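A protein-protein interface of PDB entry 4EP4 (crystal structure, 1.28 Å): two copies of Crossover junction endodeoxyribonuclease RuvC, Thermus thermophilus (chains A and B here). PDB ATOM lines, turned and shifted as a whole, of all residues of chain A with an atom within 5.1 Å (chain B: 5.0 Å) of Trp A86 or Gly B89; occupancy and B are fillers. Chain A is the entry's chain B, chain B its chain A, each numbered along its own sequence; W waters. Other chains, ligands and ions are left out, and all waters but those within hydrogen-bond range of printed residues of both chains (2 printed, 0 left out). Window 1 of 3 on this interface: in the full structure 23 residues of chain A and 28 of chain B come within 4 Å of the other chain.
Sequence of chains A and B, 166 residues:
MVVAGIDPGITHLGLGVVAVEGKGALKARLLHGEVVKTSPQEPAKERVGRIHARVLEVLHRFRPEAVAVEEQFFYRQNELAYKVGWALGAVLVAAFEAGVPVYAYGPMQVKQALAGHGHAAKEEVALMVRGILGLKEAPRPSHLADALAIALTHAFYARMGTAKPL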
ATOM      1  N   ILE A  10     -21.763  -5.635   9.655  1.00  0.00           N
ATOM      2  CA  ILE A  10     -22.612  -4.477   9.413  1.00  0.00           C
ATOM      3  C   ILE A  10     -24.050  -4.752   9.875  1.00  0.00           C
ATOM      4  O   ILE A  10     -24.662  -3.924  10.546  1.00  0.00           O
ATOM      5  CB  ILE A  10     -22.519  -3.992   7.934  1.00  0.00           C
ATOM      6  CG1 ILE A  10     -23.303  -2.699   7.733  1.00  0.00           C
ATOM      7  CG2 ILE A  10     -22.953  -5.080   6.951  1.00  0.00           C
ATOM      8  CD1 ILE A  10     -22.536  -1.459   8.154  1.00  0.00           C
ATOM      9  N   ALA A  44     -26.859   3.587   4.320  1.00  0.00           N
ATOM     10  CA  ALA A  44     -25.554   3.177   4.842  1.00  0.00           C
ATOM     11  C   ALA A  44     -25.100   4.055   6.018  1.00  0.00           C
ATOM     12  O   ALA A  44     -24.577   3.544   7.015  1.00  0.00           O
ATOM     13  CB  ALA A  44     -24.510   3.182   3.734  1.00  0.00           C
ATOM     14  N   VAL A  48     -23.975   2.710   9.819  1.00  0.00           N
ATOM     15  CA  VAL A  48     -22.639   2.990  10.334  1.00  0.00           C
ATOM     16  C   VAL A  48     -22.690   3.987  11.496  1.00  0.00           C
ATOM     17  O   VAL A  48     -21.959   3.848  12.481  1.00  0.00           O
ATOM     18  CB  VAL A  48     -21.716   3.477   9.190  1.00  0.00           C
ATOM     19  CG1 VAL A  48     -20.327   3.803   9.707  1.00  0.00           C
ATOM     20  CG2 VAL A  48     -21.639   2.419   8.103  1.00  0.00           C
ATOM     21  N   TYR A  82     -15.653  -5.320   2.342  1.00  0.00           N
ATOM     22  CA  TYR A  82     -15.827  -3.889   2.166  1.00  0.00           C
ATOM     23  C   TYR A  82     -16.787  -3.302   3.203  1.00  0.00           C
ATOM     24  O   TYR A  82     -16.477  -2.299   3.848  1.00  0.00           O
ATOM     25  CB  TYR A  82     -16.313  -3.610   0.744  1.00  0.00           C
ATOM     26  CG  TYR A  82     -16.499  -2.158   0.398  1.00  0.00           C
ATOM     27  CD1 TYR A  82     -15.477  -1.229   0.603  1.00  0.00           C
ATOM     28  CD2 TYR A  82     -17.684  -1.719  -0.178  1.00  0.00           C
ATOM     29  CE1 TYR A  82     -15.647   0.100   0.260  1.00  0.00           C
ATOM     30  CE2 TYR A  82     -17.856  -0.398  -0.525  1.00  0.00           C
ATOM     31  CZ  TYR A  82     -16.840   0.502  -0.305  1.00  0.00           C
ATOM     32  OH  TYR A  82     -17.025   1.814  -0.660  1.00  0.00           O
ATOM     33  N   LYS A  83     -17.943  -3.941   3.380  1.00  0.00           N
ATOM     34  CA  LYS A  83     -18.956  -3.438   4.302  1.00  0.00           C
ATOM     35  C   LYS A  83     -18.593  -3.669   5.767  1.00  0.00           C
ATOM     36  O   LYS A  83     -18.913  -2.845   6.624  1.00  0.00           O
ATOM     37  CB  LYS A  83     -20.319  -4.033   3.975  1.00  0.00           C
ATOM     38  CG  LYS A  83     -20.812  -3.640   2.603  1.00  0.00           C
ATOM     39  CD  LYS A  83     -22.229  -4.117   2.366  1.00  0.00           C
ATOM     40  CE  LYS A  83     -22.731  -3.623   1.026  1.00  0.00           C
ATOM     41  NZ  LYS A  83     -24.114  -4.095   0.759  1.00  0.00           N
ATOM     42  N   VAL A  84     -17.926  -4.787   6.054  1.00  0.00           N
ATOM     43  CA  VAL A  84     -17.354  -4.998   7.377  1.00  0.00           C
ATOM     44  C   VAL A  84     -16.340  -3.883   7.642  1.00  0.00           C
ATOM     45  O   VAL A  84     -16.237  -3.388   8.762  1.00  0.00           O
ATOM     46  CB  VAL A  84     -16.704  -6.390   7.502  1.00  0.00           C
ATOM     47  CG1 VAL A  84     -16.038  -6.567   8.865  1.00  0.00           C
ATOM     48  CG2 VAL A  84     -17.755  -7.472   7.286  1.00  0.00           C
ATOM     49  N   GLY A  85     -15.637  -3.462   6.591  1.00  0.00           N
ATOM     50  CA  GLY A  85     -14.753  -2.316   6.674  1.00  0.00           C
ATOM     51  C   GLY A  85     -15.456  -1.038   7.092  1.00  0.00           C
ATOM     52  O   GLY A  85     -14.911  -0.269   7.898  1.00  0.00           O
ATOM     53  N   TRP A  86     -16.652  -0.785   6.555  1.00  0.00           N
ATOM     54  CA  TRP A  86     -17.441   0.375   6.997  1.00  0.00           C
ATOM     55  C   TRP A  86     -17.636   0.340   8.507  1.00  0.00           C
ATOM     56  O   TRP A  86     -17.448   1.347   9.187  1.00  0.00           O
ATOM     57  CB  TRP A  86     -18.839   0.403   6.374  1.00  0.00           C
ATOM     58  CG  TRP A  86     -18.925   0.512   4.887  1.00  0.00           C
ATOM     59  CD1 TRP A  86     -17.898   0.675   4.003  1.00  0.00           C
ATOM     60  CD2 TRP A  86     -20.127   0.454   4.111  1.00  0.00           C
ATOM     61  NE1 TRP A  86     -18.394   0.719   2.718  1.00  0.00           N
ATOM     62  CE2 TRP A  86     -19.760   0.590   2.760  1.00  0.00           C
ATOM     63  CE3 TRP A  86     -21.482   0.285   4.430  1.00  0.00           C
ATOM     64  CZ2 TRP A  86     -20.701   0.572   1.720  1.00  0.00           C
ATOM     65  CZ3 TRP A  86     -22.420   0.275   3.398  1.00  0.00           C
ATOM     66  CH2 TRP A  86     -22.020   0.415   2.060  1.00  0.00           C
ATOM     67  N   ALA A  87     -18.026  -0.828   9.019  1.00  0.00           N
ATOM     68  CA  ALA A  87     -18.263  -1.011  10.446  1.00  0.00           C
ATOM     69  C   ALA A  87     -16.992  -0.766  11.254  1.00  0.00           C
ATOM     70  O   ALA A  87     -17.020  -0.100  12.287  1.00  0.00           O
ATOM     71  CB  ALA A  87     -18.812  -2.395  10.716  1.00  0.00           C
ATOM     72  N   LEU A  88     -15.876  -1.310  10.779  1.00  0.00           N
ATOM     73  CA  LEU A  88     -14.597  -1.106  11.447  1.00  0.00           C
ATOM     74  C   LEU A  88     -14.185   0.362  11.410  1.00  0.00           C
ATOM     75  O   LEU A  88     -13.592   0.863  12.355  1.00  0.00           O
ATOM     76  CB  LEU A  88     -13.514  -1.976  10.806  1.00  0.00           C
ATOM     77  CG  LEU A  88     -12.731  -2.880  11.752  1.00  0.00           C
ATOM     78  CD1 LEU A  88     -11.935  -2.083  12.776  1.00  0.00           C
ATOM     79  CD2 LEU A  88     -13.694  -3.810  12.453  1.00  0.00           C
ATOM     80  N   GLY A  89     -14.502   1.053  10.318  1.00  0.00           N
ATOM     81  CA  GLY A  89     -14.262   2.488  10.238  1.00  0.00           C
ATOM     82  C   GLY A  89     -14.956   3.223  11.374  1.00  0.00           C
ATOM     83  O   GLY A  89     -14.351   4.069  12.048  1.00  0.00           O
ATOM     84  N   ALA A  90     -16.219   2.873  11.610  1.00  0.00           N
ATOM     85  CA  ALA A  90     -16.985   3.443  12.718  1.00  0.00           C
ATOM     86  C   ALA A  90     -16.324   3.135  14.064  1.00  0.00           C
ATOM     87  O   ALA A  90     -16.201   4.016  14.920  1.00  0.00           O
ATOM     88  CB  ALA A  90     -18.427   2.926  12.695  1.00  0.00           C
ATOM     89  N   GLY B  85     -12.906   0.245   2.928  1.00  0.00           N
ATOM     90  CA  GLY B  85     -14.111   0.338   3.728  1.00  0.00           C
ATOM     91  C   GLY B  85     -13.942   1.187   4.976  1.00  0.00           C
ATOM     92  O   GLY B  85     -14.853   1.927   5.331  1.00  0.00           O
ATOM     93  N   TRP B  86     -12.792   1.093   5.646  1.00  0.00           N
ATOM     94  CA  TRP B  86     -12.549   1.938   6.816  1.00  0.00           C
ATOM     95  C   TRP B  86     -12.748   3.414   6.494  1.00  0.00           C
ATOM     96  O   TRP B  86     -13.382   4.147   7.263  1.00  0.00           O
ATOM     97  CB  TRP B  86     -11.117   1.797   7.326  1.00  0.00           C
ATOM     98  CG  TRP B  86     -10.722   0.475   7.870  1.00  0.00           C
ATOM     99  CD1 TRP B  86     -11.505  -0.627   8.055  1.00  0.00           C
ATOM    100  CD2 TRP B  86      -9.409   0.117   8.312  1.00  0.00           C
ATOM    101  NE1 TRP B  86     -10.749  -1.653   8.586  1.00  0.00           N
ATOM    102  CE2 TRP B  86      -9.460  -1.217   8.748  1.00  0.00           C
ATOM    103  CE3 TRP B  86      -8.190   0.797   8.365  1.00  0.00           C
ATOM    104  CZ2 TRP B  86      -8.334  -1.882   9.242  1.00  0.00           C
ATOM    105  CZ3 TRP B  86      -7.076   0.136   8.852  1.00  0.00           C
ATOM    106  CH2 TRP B  86      -7.157  -1.184   9.287  1.00  0.00           C
ATOM    107  N   ALA B  87     -12.175   3.845   5.368  1.00  0.00           N
ATOM    108  CA  ALA B  87     -12.231   5.247   4.969  1.00  0.00           C
ATOM    109  C   ALA B  87     -13.670   5.653   4.672  1.00  0.00           C
ATOM    110  O   ALA B  87     -14.119   6.729   5.081  1.00  0.00           O
ATOM    111  CB  ALA B  87     -11.334   5.493   3.763  1.00  0.00           C
ATOM    112  N   LEU B  88     -14.400   4.795   3.963  1.00  0.00           N
ATOM    113  CA  LEU B  88     -15.801   5.099   3.679  1.00  0.00           C
ATOM    114  C   LEU B  88     -16.624   5.108   4.968  1.00  0.00           C
ATOM    115  O   LEU B  88     -17.533   5.918   5.115  1.00  0.00           O
ATOM    116  CB  LEU B  88     -16.401   4.139   2.648  1.00  0.00           C
ATOM    117  CG  LEU B  88     -17.789   4.621   2.201  1.00  0.00           C
ATOM    118  CD1 LEU B  88     -17.700   5.983   1.517  1.00  0.00           C
ATOM    119  CD2 LEU B  88     -18.491   3.624   1.306  1.00  0.00           C
ATOM    120  N   GLY B  89     -16.305   4.217   5.903  1.00  0.00           N
ATOM    121  CA  GLY B  89     -16.979   4.229   7.192  1.00  0.00           C
ATOM    122  C   GLY B  89     -16.828   5.568   7.904  1.00  0.00           C
ATOM    123  O   GLY B  89     -17.801   6.105   8.456  1.00  0.00           O
ATOM    124  N   ALA B  90     -15.617   6.130   7.879  1.00  0.00           N
ATOM    125  CA  ALA B  90     -15.388   7.448   8.481  1.00  0.00           C
ATOM    126  C   ALA B  90     -16.223   8.530   7.786  1.00  0.00           C
ATOM    127  O   ALA B  90     -16.809   9.395   8.440  1.00  0.00           O
ATOM    128  CB  ALA B  90     -13.912   7.809   8.456  1.00  0.00           C
ATOM    129  N   VAL B  91     -16.279   8.477   6.457  1.00  0.00           N
ATOM    130  CA  VAL B  91     -17.100   9.398   5.680  1.00  0.00           C
ATOM    131  C   VAL B  91     -18.575   9.280   6.067  1.00  0.00           C
ATOM    132  O   VAL B  91     -19.255  10.285   6.256  1.00  0.00           O
ATOM    133  CB  VAL B  91     -16.944   9.115   4.179  1.00  0.00           C
ATOM    134  CG1 VAL B  91     -17.970   9.888   3.383  1.00  0.00           C
ATOM    135  CG2 VAL B  91     -15.529   9.451   3.722  1.00  0.00           C
ATOM    136  N   LEU B  92     -19.049   8.043   6.213  1.00  0.00           N
ATOM    137  CA  LEU B  92     -20.441   7.796   6.567  1.00  0.00           C
ATOM    138  C   LEU B  92     -20.791   8.304   7.967  1.00  0.00           C
ATOM    139  O   LEU B  92     -21.876   8.858   8.165  1.00  0.00           O
ATOM    140  CB  LEU B  92     -20.778   6.310   6.417  1.00  0.00           C
ATOM    141  CG  LEU B  92     -20.781   5.805   4.969  1.00  0.00           C
ATOM    142  CD1 LEU B  92     -20.883   4.292   4.943  1.00  0.00           C
ATOM    143  CD2 LEU B  92     -21.919   6.423   4.168  1.00  0.00           C
ATOM    144  N   VAL B  93     -19.891   8.121   8.935  1.00  0.00           N
ATOM    145  CA  VAL B  93     -20.129   8.684  10.268  1.00  0.00           C
ATOM    146  C   VAL B  93     -20.257  10.212  10.167  1.00  0.00           C
ATOM    147  O   VAL B  93     -21.175  10.800  10.746  1.00  0.00           O
ATOM    148  CB  VAL B  93     -19.043   8.311  11.300  1.00  0.00           C
ATOM    149  CG1 VAL B  93     -19.323   9.013  12.625  1.00  0.00           C
ATOM    150  CG2 VAL B  93     -18.968   6.798  11.484  1.00  0.00           C
ATOM    151  N   LEU B 166     -27.017   5.667  -1.311  1.00  0.00           N
ATOM    152  CA  LEU B 166     -26.168   4.604  -0.770  1.00  0.00           C
ATOM    153  C   LEU B 166     -26.773   3.965   0.491  1.00  0.00           C
ATOM    154  O   LEU B 166     -27.078   4.638   1.485  1.00  0.00           O
ATOM    155  CB  LEU B 166     -24.748   5.122  -0.485  1.00  0.00           C
ATOM    156  CG  LEU B 166     -23.761   4.095   0.088  1.00  0.00           C
ATOM    157  CD1 LEU B 166     -23.520   2.941  -0.877  1.00  0.00           C
ATOM    158  CD2 LEU B 166     -22.447   4.748   0.494  1.00  0.00           C
ATOM    159  OXT LEU B 166     -26.962   2.743   0.550  1.00  0.00           O
HETATM  160  O   HOH W   1     -26.013   6.604   3.372  1.00  0.00           O
HETATM  161  O   HOH W   2     -28.091   1.116   2.451  1.00  0.00           O
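The backbone carbonyl oxygen (O) of Gly B85 sits close to the backbone NH (N) of Trp A86 (3.5 Å).
The backbone NH of Trp B86 lies within hydrogen-bond range of the backbone carbonyl oxygen of Gly A85, 3.4 Å away.
O of Leu B166 lies within hydrogen-bond range of N of Ala A44 (3.0 Å).
O of Gly A85 lies close to O of Gly B85 (3.4 Å).
Val A48 touches Gly B89.
CG2 of Val A48 touches CD1 of Leu B92, 3.8 Å away.
Val A48 touches Val B93 (CG1 to CG2, 3.7 Å).
Gly B85 touches Tyr A82 (CA to O, 3.5 Å).
Leu B88 touches Tyr A82.
Trp A86 touches Leu B88 (NE1 to CD2, 3.2 Å).
Gly B89 touches Trp A86.
Trp A86 touches Leu B92 (CD2 to CD1, 3.999 Å).
NE1 of Trp B86 touches CB of Leu A88 (3.6 Å).
Trp B86 touches Gly A89 (O to CA, 3.5 Å).
Of the printed residues of chain B, Trp A86 touches Gly B85 (3.4 Å), Leu B88 (3.2 Å), Gly B89 (3.5 Å) and Leu B92 (3.999 Å).
Of chain A, only Val A48 and Trp A86 come within 4 Å of Gly B89.
Of the printed residues of chain A, Gly B85 touches Tyr A82, Gly A85 and Trp A86.
Of the printed residues of chain A, Trp B86 touches Gly A85, Leu A88 and Gly A89.
Of the printed residues of chain B, Gly A85 touches Gly B85 and Trp B86.
Printed residues of chain A within 4 Å of Leu B88: Tyr A82 (3.0 Å) and Trp A86 (3.2 Å).
Ile A10 touches none of the printed residues of chain B.
Printed residues of chain A that touch a printed residue of chain B: Ala A44, Val A48, Tyr A82, Gly A85, Trp A86, Leu A88 and Gly A89.
Printed residues of chain B that touch a printed residue of chain A: Gly B85, Trp B86, Leu B88, Gly B89, Leu B92, Val B93 and Leu B166.
Among the printed residues, no Asp or Glu carboxylate lies within 4 Å of a Lys or Arg side-chain nitrogen of the other chain.
Gly A85 touches its own counterpart, Gly B85.
Gly A85 touches Trp B86, and with the chains exchanged Trp A86 touches Gly B85.
Trp A86 touches Leu B88, and with the chains exchanged Leu A88 touches Trp B86.
Trp A86 touches Gly B89, and with the chains exchanged Gly A89 touches Trp B86.
Positions printed for both chains: 85, 86, 87, 88, 89 and 90.
Of the 15 pairs that touch across the chains among the printed residues, 7 have their exchanged pair printed and touching as well.
Water W2 lies within hydrogen-bond range of the chain-end carboxylate (OXT) of Leu B166 (2.7 Å) and the backbone NH (N) of Ala A44 (3.3 Å).
Water W1 bridges the chain-end carboxylate of Leu B166 and the backbone NH of Ala A44.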
